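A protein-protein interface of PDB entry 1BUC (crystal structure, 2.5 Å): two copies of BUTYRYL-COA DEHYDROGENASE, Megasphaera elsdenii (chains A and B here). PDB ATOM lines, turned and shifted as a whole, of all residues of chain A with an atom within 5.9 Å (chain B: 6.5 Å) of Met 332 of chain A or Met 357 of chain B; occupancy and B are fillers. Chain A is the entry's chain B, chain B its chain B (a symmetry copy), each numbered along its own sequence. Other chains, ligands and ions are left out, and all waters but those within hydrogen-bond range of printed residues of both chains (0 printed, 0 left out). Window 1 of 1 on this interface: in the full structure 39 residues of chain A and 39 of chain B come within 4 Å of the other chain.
The backbone carbonyl oxygen (O) of Thr 336 of chain A sits at hydrogen-bond distance from the side-chain amino group (NZ) of Lys 361 of chain B. The side-chain amino group of Lys 361 of chain A is in hydrogen-bond range of the backbone carbonyl oxygen of Thr 336 of chain B, at 3.3 Å.
OG1 of Thr 336 of chain A sits at hydrogen-bond distance from O of Met 332 of chain A, at 2.9 Å. The side-chain sulfur (SD) of Met 332 of chain A sits close to the side-chain amide oxygen (OE1) of Gln 364 of chain A, at 3.5 Å. N of Met 357 of chain A lies within hydrogen-bond range of OG1 of Thr 335 of chain A, 2.8 Å away. The side-chain amino group of Lys 361 of chain A lies within hydrogen-bond range of the side-chain amide oxygen of Gln 364 of chain A, at 3.0 Å. The side-chain hydroxyl of Thr 336 of chain B sits at hydrogen-bond distance from the backbone carbonyl oxygen of Met 332 of chain B, at 2.9 Å. The side-chain hydroxyl of Thr 335 of chain B is in hydrogen-bond range of the backbone NH of Met 357 of chain B (2.8 Å).
Among the printed residues, pairs that only touch across the chains: Met 206 of chain A with Ala 354 of chain B, Met 206 of chain A with Met 357 of chain B, Met 206 of chain A with Arg 358 of chain B, Met 332 of chain A with Met 357 of chain B, Met 357 of chain A with Met 206 of chain B, Met 357 of chain A with Met 332 of chain B, Arg 358 of chain A with Met 206 of chain B and Lys 361 of chain A with Val 339 of chain B.
Printed residues of chain B within 4 Å of Thr 336 of chain A: Lys 361. Of the printed residues of chain B, Arg 358 of chain A touches Met 206 (3.8 Å). Of the printed residues of chain A, Val 339 of chain B touches Lys 361. Met 357 of chain B touches two residues of chain A. Of the printed residues of chain A, Lys 361 of chain B touches Thr 336 (3.3 Å). The nearest printed residue of chain A that does not touch Ala 354 of chain B is Lys 361 of chain A (7.6 Å).
Hydrophobic or aromatic side chains of chain A within 4 Å of the printed part of chain B: Met 206, Met 332 and Met 357.
Met 206 of chain A touches Met 357 of chain B, and with the chains exchanged Met 357 of chain A touches Met 206 of chain B. Met 206 of chain A touches Arg 358 of chain B, and with the chains exchanged Arg 358 of chain A touches Met 206 of chain B. Met 332 of chain A touches Met 357 of chain B, and with the chains exchanged Met 357 of chain A touches Met 332 of chain B. Thr 336 of chain A touches Lys 361 of chain B, and with the chains exchanged Lys 361 of chain A touches Thr 336 of chain B. Of the 10 pairs that touch across the chains among the printed residues, 8 have their exchanged pair printed and touching as well.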
ATOM      1  N   MET A 206      -5.007 -14.212  12.105  1.00  0.00           N
ATOM      2  CA  MET A 206      -5.804 -14.579  10.931  1.00  0.00           C
ATOM      3  C   MET A 206      -6.767 -13.487  10.475  1.00  0.00           C
ATOM      4  O   MET A 206      -7.006 -13.315   9.279  1.00  0.00           O
ATOM      5  CB  MET A 206      -6.586 -15.868  11.224  1.00  0.00           C
ATOM      6  CG  MET A 206      -7.582 -16.283  10.149  1.00  0.00           C
ATOM      7  SD  MET A 206      -8.764 -17.489  10.764  1.00  0.00           S
ATOM      8  CE  MET A 206      -8.446 -18.866   9.717  1.00  0.00           C
ATOM      9  N   ALA A 327     -23.617 -16.176  20.770  1.00  0.00           N
ATOM     10  CA  ALA A 327     -23.230 -15.099  19.870  1.00  0.00           C
ATOM     11  C   ALA A 327     -22.048 -15.494  18.985  1.00  0.00           C
ATOM     12  O   ALA A 327     -22.098 -15.303  17.767  1.00  0.00           O
ATOM     13  CB  ALA A 327     -22.906 -13.842  20.651  1.00  0.00           C
ATOM     14  N   SER A 328     -20.997 -16.062  19.578  1.00  0.00           N
ATOM     15  CA  SER A 328     -19.823 -16.433  18.797  1.00  0.00           C
ATOM     16  C   SER A 328     -20.134 -17.482  17.739  1.00  0.00           C
ATOM     17  O   SER A 328     -19.686 -17.373  16.594  1.00  0.00           O
ATOM     18  CB  SER A 328     -18.668 -16.889  19.698  1.00  0.00           C
ATOM     19  OG  SER A 328     -19.098 -17.769  20.714  1.00  0.00           O
ATOM     20  N   ASP A 329     -20.932 -18.480  18.107  1.00  0.00           N
ATOM     21  CA  ASP A 329     -21.301 -19.539  17.173  1.00  0.00           C
ATOM     22  C   ASP A 329     -22.157 -18.987  16.037  1.00  0.00           C
ATOM     23  O   ASP A 329     -21.940 -19.320  14.870  1.00  0.00           O
ATOM     24  CB  ASP A 329     -22.040 -20.669  17.894  1.00  0.00           C
ATOM     25  CG  ASP A 329     -21.165 -21.400  18.906  1.00  0.00           C
ATOM     26  OD1 ASP A 329     -19.925 -21.407  18.751  1.00  0.00           O
ATOM     27  OD2 ASP A 329     -21.726 -21.981  19.859  1.00  0.00           O
ATOM     28  N   VAL A 330     -23.131 -18.146  16.376  1.00  0.00           N
ATOM     29  CA  VAL A 330     -23.950 -17.500  15.361  1.00  0.00           C
ATOM     30  C   VAL A 330     -23.042 -16.743  14.399  1.00  0.00           C
ATOM     31  O   VAL A 330     -23.114 -16.944  13.186  1.00  0.00           O
ATOM     32  CB  VAL A 330     -24.980 -16.529  15.981  1.00  0.00           C
ATOM     33  CG1 VAL A 330     -25.517 -15.564  14.920  1.00  0.00           C
ATOM     34  CG2 VAL A 330     -26.126 -17.318  16.591  1.00  0.00           C
ATOM     35  N   ALA A 331     -22.160 -15.915  14.947  1.00  0.00           N
ATOM     36  CA  ALA A 331     -21.235 -15.136  14.139  1.00  0.00           C
ATOM     37  C   ALA A 331     -20.546 -16.023  13.119  1.00  0.00           C
ATOM     38  O   ALA A 331     -20.537 -15.705  11.931  1.00  0.00           O
ATOM     39  CB  ALA A 331     -20.207 -14.449  15.020  1.00  0.00           C
ATOM     40  N   MET A 332     -20.020 -17.157  13.572  1.00  0.00           N
ATOM     41  CA  MET A 332     -19.326 -18.085  12.685  1.00  0.00           C
ATOM     42  C   MET A 332     -20.234 -18.714  11.617  1.00  0.00           C
ATOM     43  O   MET A 332     -19.828 -18.841  10.460  1.00  0.00           O
ATOM     44  CB  MET A 332     -18.629 -19.177  13.495  1.00  0.00           C
ATOM     45  CG  MET A 332     -17.493 -19.871  12.752  1.00  0.00           C
ATOM     46  SD  MET A 332     -16.036 -18.826  12.529  1.00  0.00           S
ATOM     47  CE  MET A 332     -16.127 -18.519  10.782  1.00  0.00           C
ATOM     48  N   ARG A 333     -21.453 -19.097  11.997  1.00  0.00           N
ATOM     49  CA  ARG A 333     -22.425 -19.676  11.058  1.00  0.00           C
ATOM     50  C   ARG A 333     -22.849 -18.657  10.009  1.00  0.00           C
ATOM     51  O   ARG A 333     -22.716 -18.886   8.810  1.00  0.00           O
ATOM     52  CB  ARG A 333     -23.685 -20.138  11.799  1.00  0.00           C
ATOM     53  CG  ARG A 333     -23.552 -21.411  12.628  1.00  0.00           C
ATOM     54  CD  ARG A 333     -24.379 -22.545  12.019  1.00  0.00           C
ATOM     55  NE  ARG A 333     -25.746 -22.128  11.685  1.00  0.00           N
ATOM     56  CZ  ARG A 333     -26.254 -22.114  10.451  1.00  0.00           C
ATOM     57  NH1 ARG A 333     -25.519 -22.492   9.409  1.00  0.00           N
ATOM     58  NH2 ARG A 333     -27.510 -21.731  10.259  1.00  0.00           N
ATOM     59  N   VAL A 334     -23.396 -17.543  10.486  1.00  0.00           N
ATOM     60  CA  VAL A 334     -23.866 -16.451   9.646  1.00  0.00           C
ATOM     61  C   VAL A 334     -22.773 -15.905   8.732  1.00  0.00           C
ATOM     62  O   VAL A 334     -23.005 -15.632   7.550  1.00  0.00           O
ATOM     63  CB  VAL A 334     -24.428 -15.317  10.523  1.00  0.00           C
ATOM     64  CG1 VAL A 334     -24.770 -14.095   9.686  1.00  0.00           C
ATOM     65  CG2 VAL A 334     -25.656 -15.815  11.251  1.00  0.00           C
ATOM     66  N   THR A 335     -21.568 -15.786   9.268  1.00  0.00           N
ATOM     67  CA  THR A 335     -20.467 -15.258   8.489  1.00  0.00           C
ATOM     68  C   THR A 335     -20.058 -16.209   7.357  1.00  0.00           C
ATOM     69  O   THR A 335     -19.870 -15.773   6.220  1.00  0.00           O
ATOM     70  CB  THR A 335     -19.271 -14.876   9.398  1.00  0.00           C
ATOM     71  OG1 THR A 335     -18.461 -13.911   8.725  1.00  0.00           O
ATOM     72  CG2 THR A 335     -18.425 -16.077   9.753  1.00  0.00           C
ATOM     73  N   THR A 336     -20.009 -17.508   7.642  1.00  0.00           N
ATOM     74  CA  THR A 336     -19.619 -18.487   6.634  1.00  0.00           C
ATOM     75  C   THR A 336     -20.664 -18.569   5.522  1.00  0.00           C
ATOM     76  O   THR A 336     -20.311 -18.706   4.349  1.00  0.00           O
ATOM     77  CB  THR A 336     -19.362 -19.883   7.256  1.00  0.00           C
ATOM     78  OG1 THR A 336     -18.252 -19.807   8.164  1.00  0.00           O
ATOM     79  CG2 THR A 336     -19.041 -20.901   6.180  1.00  0.00           C
ATOM     80  N   GLU A 337     -21.940 -18.437   5.887  1.00  0.00           N
ATOM     81  CA  GLU A 337     -23.021 -18.423   4.902  1.00  0.00           C
ATOM     82  C   GLU A 337     -22.907 -17.177   4.004  1.00  0.00           C
ATOM     83  O   GLU A 337     -23.024 -17.269   2.776  1.00  0.00           O
ATOM     84  CB  GLU A 337     -24.405 -18.484   5.586  1.00  0.00           C
ATOM     85  CG  GLU A 337     -24.721 -19.815   6.318  1.00  0.00           C
ATOM     86  CD  GLU A 337     -26.155 -19.893   6.892  1.00  0.00           C
ATOM     87  OE1 GLU A 337     -27.117 -20.058   6.110  1.00  0.00           O
ATOM     88  OE2 GLU A 337     -26.323 -19.813   8.129  1.00  0.00           O
ATOM     89  N   MET A 357     -15.768 -13.176   8.176  1.00  0.00           N
ATOM     90  CA  MET A 357     -15.589 -14.581   8.488  1.00  0.00           C
ATOM     91  C   MET A 357     -14.302 -14.797   9.269  1.00  0.00           C
ATOM     92  O   MET A 357     -14.291 -15.508  10.275  1.00  0.00           O
ATOM     93  CB  MET A 357     -15.586 -15.405   7.208  1.00  0.00           C
ATOM     94  CG  MET A 357     -15.401 -16.886   7.432  1.00  0.00           C
ATOM     95  SD  MET A 357     -15.644 -17.809   5.919  1.00  0.00           S
ATOM     96  CE  MET A 357     -14.719 -19.276   6.318  1.00  0.00           C
ATOM     97  N   ARG A 358     -13.224 -14.154   8.825  1.00  0.00           N
ATOM     98  CA  ARG A 358     -11.948 -14.249   9.522  1.00  0.00           C
ATOM     99  C   ARG A 358     -12.055 -13.738  10.952  1.00  0.00           C
ATOM    100  O   ARG A 358     -11.500 -14.336  11.872  1.00  0.00           O
ATOM    101  CB  ARG A 358     -10.854 -13.493   8.765  1.00  0.00           C
ATOM    102  CG  ARG A 358     -10.384 -14.218   7.507  1.00  0.00           C
ATOM    103  CD  ARG A 358      -9.129 -13.598   6.906  1.00  0.00           C
ATOM    104  NE  ARG A 358      -9.398 -12.372   6.157  1.00  0.00           N
ATOM    105  CZ  ARG A 358      -9.270 -11.144   6.648  1.00  0.00           C
ATOM    106  NH1 ARG A 358      -8.875 -10.951   7.905  1.00  0.00           N
ATOM    107  NH2 ARG A 358      -9.541 -10.104   5.877  1.00  0.00           N
ATOM    108  N   ALA A 360     -14.915 -13.473  12.878  1.00  0.00           N
ATOM    109  CA  ALA A 360     -15.816 -14.298  13.674  1.00  0.00           C
ATOM    110  C   ALA A 360     -15.078 -15.334  14.516  1.00  0.00           C
ATOM    111  O   ALA A 360     -15.419 -15.548  15.676  1.00  0.00           O
ATOM    112  CB  ALA A 360     -16.823 -14.987  12.778  1.00  0.00           C
ATOM    113  N   LYS A 361     -14.022 -15.915  13.957  1.00  0.00           N
ATOM    114  CA  LYS A 361     -13.304 -16.997  14.624  1.00  0.00           C
ATOM    115  C   LYS A 361     -12.700 -16.716  16.006  1.00  0.00           C
ATOM    116  O   LYS A 361     -12.720 -17.596  16.865  1.00  0.00           O
ATOM    117  CB  LYS A 361     -12.251 -17.608  13.692  1.00  0.00           C
ATOM    118  CG  LYS A 361     -11.692 -18.917  14.216  1.00  0.00           C
ATOM    119  CD  LYS A 361     -12.833 -19.883  14.538  1.00  0.00           C
ATOM    120  CE  LYS A 361     -12.415 -20.963  15.520  1.00  0.00           C
ATOM    121  NZ  LYS A 361     -13.542 -21.873  15.841  1.00  0.00           N
ATOM    122  N   THR A 363     -13.871 -14.860  18.347  1.00  0.00           N
ATOM    123  CA  THR A 363     -14.923 -14.737  19.344  1.00  0.00           C
ATOM    124  C   THR A 363     -15.287 -16.076  20.001  1.00  0.00           C
ATOM    125  O   THR A 363     -15.911 -16.100  21.057  1.00  0.00           O
ATOM    126  CB  THR A 363     -16.186 -14.071  18.757  1.00  0.00           C
ATOM    127  OG1 THR A 363     -16.860 -14.985  17.883  1.00  0.00           O
ATOM    128  CG2 THR A 363     -15.813 -12.806  17.987  1.00  0.00           C
ATOM    129  N   GLN A 364     -14.888 -17.181  19.380  1.00  0.00           N
ATOM    130  CA  GLN A 364     -15.126 -18.509  19.940  1.00  0.00           C
ATOM    131  C   GLN A 364     -13.957 -18.954  20.816  1.00  0.00           C
ATOM    132  O   GLN A 364     -14.015 -20.004  21.467  1.00  0.00           O
ATOM    133  CB  GLN A 364     -15.315 -19.521  18.811  1.00  0.00           C
ATOM    134  CG  GLN A 364     -16.379 -19.131  17.815  1.00  0.00           C
ATOM    135  CD  GLN A 364     -16.652 -20.216  16.802  1.00  0.00           C
ATOM    136  OE1 GLN A 364     -16.095 -20.216  15.706  1.00  0.00           O
ATOM    137  NE2 GLN A 364     -17.525 -21.148  17.160  1.00  0.00           N
ATOM    138  N   MET B 206      -8.834 -14.721  -0.184  1.00  0.00           N
ATOM    139  CA  MET B 206      -8.836 -14.950   1.263  1.00  0.00           C
ATOM    140  C   MET B 206      -7.864 -16.035   1.716  1.00  0.00           C
ATOM    141  O   MET B 206      -7.268 -15.940   2.790  1.00  0.00           O
ATOM    142  CB  MET B 206     -10.258 -15.306   1.725  1.00  0.00           C
ATOM    143  CG  MET B 206     -10.381 -15.727   3.184  1.00  0.00           C
ATOM    144  SD  MET B 206     -11.938 -16.565   3.506  1.00  0.00           S
ATOM    145  CE  MET B 206     -12.676 -15.502   4.697  1.00  0.00           C
ATOM    146  N   ILE B 257      -7.448 -31.110   2.534  1.00  0.00           N
ATOM    147  CA  ILE B 257      -7.376 -29.999   3.480  1.00  0.00           C
ATOM    148  C   ILE B 257      -7.902 -30.441   4.842  1.00  0.00           C
ATOM    149  O   ILE B 257      -7.340 -30.083   5.886  1.00  0.00           O
ATOM    150  CB  ILE B 257      -8.190 -28.782   2.985  1.00  0.00           C
ATOM    151  CG1 ILE B 257      -7.608 -28.267   1.669  1.00  0.00           C
ATOM    152  CG2 ILE B 257      -8.157 -27.671   4.019  1.00  0.00           C
ATOM    153  CD1 ILE B 257      -8.460 -27.236   0.980  1.00  0.00           C
ATOM    154  N   ALA B 331     -14.849 -30.313   4.905  1.00  0.00           N
ATOM    155  CA  ALA B 331     -13.644 -29.502   4.984  1.00  0.00           C
ATOM    156  C   ALA B 331     -13.884 -28.280   5.850  1.00  0.00           C
ATOM    157  O   ALA B 331     -13.113 -28.016   6.771  1.00  0.00           O
ATOM    158  CB  ALA B 331     -13.191 -29.084   3.596  1.00  0.00           C
ATOM    159  N   MET B 332     -14.978 -27.570   5.592  1.00  0.00           N
ATOM    160  CA  MET B 332     -15.308 -26.371   6.354  1.00  0.00           C
ATOM    161  C   MET B 332     -15.609 -26.644   7.837  1.00  0.00           C
ATOM    162  O   MET B 332     -15.170 -25.886   8.704  1.00  0.00           O
ATOM    163  CB  MET B 332     -16.477 -25.631   5.706  1.00  0.00           C
ATOM    164  CG  MET B 332     -16.571 -24.159   6.093  1.00  0.00           C
ATOM    165  SD  MET B 332     -15.265 -23.141   5.370  1.00  0.00           S
ATOM    166  CE  MET B 332     -14.295 -22.792   6.816  1.00  0.00           C
ATOM    167  N   THR B 335     -12.297 -28.095   9.509  1.00  0.00           N
ATOM    168  CA  THR B 335     -11.293 -27.052   9.567  1.00  0.00           C
ATOM    169  C   THR B 335     -11.599 -26.023  10.664  1.00  0.00           C
ATOM    170  O   THR B 335     -10.708 -25.655  11.431  1.00  0.00           O
ATOM    171  CB  THR B 335     -11.092 -26.391   8.179  1.00  0.00           C
ATOM    172  OG1 THR B 335      -9.799 -25.786   8.132  1.00  0.00           O
ATOM    173  CG2 THR B 335     -12.143 -25.344   7.894  1.00  0.00           C
ATOM    174  N   THR B 336     -12.864 -25.632  10.795  1.00  0.00           N
ATOM    175  CA  THR B 336     -13.249 -24.650  11.801  1.00  0.00           C
ATOM    176  C   THR B 336     -13.071 -25.215  13.210  1.00  0.00           C
ATOM    177  O   THR B 336     -12.645 -24.497  14.116  1.00  0.00           O
ATOM    178  CB  THR B 336     -14.698 -24.144  11.587  1.00  0.00           C
ATOM    179  OG1 THR B 336     -14.786 -23.457  10.330  1.00  0.00           O
ATOM    180  CG2 THR B 336     -15.104 -23.189  12.692  1.00  0.00           C
ATOM    181  N   GLU B 337     -13.350 -26.508  13.377  1.00  0.00           N
ATOM    182  CA  GLU B 337     -13.145 -27.176  14.662  1.00  0.00           C
ATOM    183  C   GLU B 337     -11.644 -27.217  15.008  1.00  0.00           C
ATOM    184  O   GLU B 337     -11.247 -26.916  16.140  1.00  0.00           O
ATOM    185  CB  GLU B 337     -13.748 -28.599  14.658  1.00  0.00           C
ATOM    186  CG  GLU B 337     -15.296 -28.659  14.564  1.00  0.00           C
ATOM    187  CD  GLU B 337     -15.878 -30.087  14.681  1.00  0.00           C
ATOM    188  OE1 GLU B 337     -15.893 -30.650  15.797  1.00  0.00           O
ATOM    189  OE2 GLU B 337     -16.346 -30.641  13.661  1.00  0.00           O
ATOM    190  N   VAL B 339      -9.134 -25.176  14.286  1.00  0.00           N
ATOM    191  CA  VAL B 339      -8.676 -23.897  14.823  1.00  0.00           C
ATOM    192  C   VAL B 339      -9.053 -23.793  16.302  1.00  0.00           C
ATOM    193  O   VAL B 339      -8.235 -23.393  17.132  1.00  0.00           O
ATOM    194  CB  VAL B 339      -9.283 -22.681  14.054  1.00  0.00           C
ATOM    195  CG1 VAL B 339      -8.682 -21.390  14.567  1.00  0.00           C
ATOM    196  CG2 VAL B 339      -9.045 -22.804  12.559  1.00  0.00           C
ATOM    197  N   PRO B 352      -0.376 -23.907  11.073  1.00  0.00           N
ATOM    198  CA  PRO B 352      -0.973 -24.367   9.812  1.00  0.00           C
ATOM    199  C   PRO B 352      -2.495 -24.421   9.823  1.00  0.00           C
ATOM    200  O   PRO B 352      -3.147 -24.491   8.773  1.00  0.00           O
ATOM    201  CB  PRO B 352      -0.384 -25.766   9.664  1.00  0.00           C
ATOM    202  CG  PRO B 352      -0.358 -26.240  11.081  1.00  0.00           C
ATOM    203  CD  PRO B 352       0.196 -25.043  11.822  1.00  0.00           C
ATOM    204  N   VAL B 353      -3.058 -24.383  11.018  1.00  0.00           N
ATOM    205  CA  VAL B 353      -4.476 -24.588  11.190  1.00  0.00           C
ATOM    206  C   VAL B 353      -5.341 -23.450  10.624  1.00  0.00           C
ATOM    207  O   VAL B 353      -6.373 -23.705   9.997  1.00  0.00           O
ATOM    208  CB  VAL B 353      -4.766 -24.946  12.670  1.00  0.00           C
ATOM    209  CG1 VAL B 353      -5.784 -24.035  13.280  1.00  0.00           C
ATOM    210  CG2 VAL B 353      -5.187 -26.397  12.771  1.00  0.00           C
ATOM    211  N   ALA B 354      -4.874 -22.211  10.748  1.00  0.00           N
ATOM    212  CA  ALA B 354      -5.620 -21.060  10.238  1.00  0.00           C
ATOM    213  C   ALA B 354      -5.717 -21.113   8.713  1.00  0.00           C
ATOM    214  O   ALA B 354      -6.796 -20.931   8.133  1.00  0.00           O
ATOM    215  CB  ALA B 354      -4.959 -19.756  10.684  1.00  0.00           C
ATOM    216  N   ARG B 355      -4.586 -21.399   8.077  1.00  0.00           N
ATOM    217  CA  ARG B 355      -4.492 -21.507   6.628  1.00  0.00           C
ATOM    218  C   ARG B 355      -5.541 -22.471   6.086  1.00  0.00           C
ATOM    219  O   ARG B 355      -6.257 -22.157   5.130  1.00  0.00           O
ATOM    220  CB  ARG B 355      -3.100 -22.013   6.242  1.00  0.00           C
ATOM    221  CG  ARG B 355      -2.716 -21.766   4.803  1.00  0.00           C
ATOM    222  CD  ARG B 355      -1.358 -22.362   4.498  1.00  0.00           C
ATOM    223  NE  ARG B 355      -1.442 -23.763   4.100  1.00  0.00           N
ATOM    224  CZ  ARG B 355      -0.796 -24.757   4.700  1.00  0.00           C
ATOM    225  NH1 ARG B 355      -0.017 -24.520   5.751  1.00  0.00           N
ATOM    226  NH2 ARG B 355      -0.893 -25.989   4.218  1.00  0.00           N
ATOM    227  N   HIS B 356      -5.631 -23.640   6.710  1.00  0.00           N
ATOM    228  CA  HIS B 356      -6.554 -24.680   6.269  1.00  0.00           C
ATOM    229  C   HIS B 356      -7.997 -24.194   6.241  1.00  0.00           C
ATOM    230  O   HIS B 356      -8.723 -24.456   5.286  1.00  0.00           O
ATOM    231  CB  HIS B 356      -6.423 -25.918   7.161  1.00  0.00           C
ATOM    232  CG  HIS B 356      -5.068 -26.546   7.114  1.00  0.00           C
ATOM    233  ND1 HIS B 356      -4.441 -27.064   8.228  1.00  0.00           N
ATOM    234  CD2 HIS B 356      -4.202 -26.710   6.089  1.00  0.00           C
ATOM    235  CE1 HIS B 356      -3.248 -27.518   7.888  1.00  0.00           C
ATOM    236  NE2 HIS B 356      -3.079 -27.315   6.596  1.00  0.00           N
ATOM    237  N   MET B 357      -8.396 -23.463   7.279  1.00  0.00           N
ATOM    238  CA  MET B 357      -9.741 -22.929   7.366  1.00  0.00           C
ATOM    239  C   MET B 357     -10.003 -21.947   6.234  1.00  0.00           C
ATOM    240  O   MET B 357     -11.046 -22.007   5.582  1.00  0.00           O
ATOM    241  CB  MET B 357      -9.952 -22.259   8.718  1.00  0.00           C
ATOM    242  CG  MET B 357     -11.328 -21.668   8.902  1.00  0.00           C
ATOM    243  SD  MET B 357     -11.579 -21.115  10.584  1.00  0.00           S
ATOM    244  CE  MET B 357     -12.871 -19.921  10.310  1.00  0.00           C
ATOM    245  N   ARG B 358      -9.038 -21.066   5.980  1.00  0.00           N
ATOM    246  CA  ARG B 358      -9.160 -20.109   4.887  1.00  0.00           C
ATOM    247  C   ARG B 358      -9.310 -20.812   3.545  1.00  0.00           C
ATOM    248  O   ARG B 358     -10.112 -20.398   2.709  1.00  0.00           O
ATOM    249  CB  ARG B 358      -7.964 -19.155   4.860  1.00  0.00           C
ATOM    250  CG  ARG B 358      -8.004 -18.110   5.970  1.00  0.00           C
ATOM    251  CD  ARG B 358      -6.962 -17.015   5.786  1.00  0.00           C
ATOM    252  NE  ARG B 358      -5.615 -17.436   6.166  1.00  0.00           N
ATOM    253  CZ  ARG B 358      -4.696 -17.882   5.316  1.00  0.00           C
ATOM    254  NH1 ARG B 358      -4.961 -17.978   4.014  1.00  0.00           N
ATOM    255  NH2 ARG B 358      -3.506 -18.235   5.773  1.00  0.00           N
ATOM    256  N   ASP B 359      -8.564 -21.895   3.357  1.00  0.00           N
ATOM    257  CA  ASP B 359      -8.613 -22.657   2.112  1.00  0.00           C
ATOM    258  C   ASP B 359      -9.938 -23.386   1.926  1.00  0.00           C
ATOM    259  O   ASP B 359     -10.516 -23.359   0.846  1.00  0.00           O
ATOM    260  CB  ASP B 359      -7.470 -23.678   2.056  1.00  0.00           C
ATOM    261  CG  ASP B 359      -6.098 -23.030   2.009  1.00  0.00           C
ATOM    262  OD1 ASP B 359      -6.005 -21.796   1.832  1.00  0.00           O
ATOM    263  OD2 ASP B 359      -5.103 -23.765   2.147  1.00  0.00           O
ATOM    264  N   ALA B 360     -10.417 -24.038   2.978  1.00  0.00           N
ATOM    265  CA  ALA B 360     -11.654 -24.809   2.913  1.00  0.00           C
ATOM    266  C   ALA B 360     -12.778 -24.062   2.203  1.00  0.00           C
ATOM    267  O   ALA B 360     -13.510 -24.648   1.410  1.00  0.00           O
ATOM    268  CB  ALA B 360     -12.097 -25.203   4.305  1.00  0.00           C
ATOM    269  N   LYS B 361     -12.862 -22.755   2.429  1.00  0.00           N
ATOM    270  CA  LYS B 361     -13.960 -21.956   1.893  1.00  0.00           C
ATOM    271  C   LYS B 361     -14.157 -21.934   0.371  1.00  0.00           C
ATOM    272  O   LYS B 361     -15.297 -21.919  -0.091  1.00  0.00           O
ATOM    273  CB  LYS B 361     -13.919 -20.529   2.449  1.00  0.00           C
ATOM    274  CG  LYS B 361     -15.192 -19.753   2.170  1.00  0.00           C
ATOM    275  CD  LYS B 361     -16.406 -20.545   2.654  1.00  0.00           C
ATOM    276  CE  LYS B 361     -17.690 -20.112   1.969  1.00  0.00           C
ATOM    277  NZ  LYS B 361     -18.852 -20.910   2.432  1.00  0.00           N
ATOM    278  N   ILE B 362     -13.093 -21.949  -0.427  1.00  0.00           N
ATOM    279  CA  ILE B 362     -13.316 -21.927  -1.881  1.00  0.00           C
ATOM    280  C   ILE B 362     -13.936 -23.197  -2.406  1.00  0.00           C
ATOM    281  O   ILE B 362     -14.617 -23.167  -3.428  1.00  0.00           O
ATOM    282  CB  ILE B 362     -12.052 -21.651  -2.751  1.00  0.00           C
ATOM    283  CG1 ILE B 362     -10.762 -21.988  -2.010  1.00  0.00           C
ATOM    284  CG2 ILE B 362     -12.128 -20.273  -3.358  1.00  0.00           C
ATOM    285  CD1 ILE B 362     -10.415 -23.457  -2.051  1.00  0.00           C
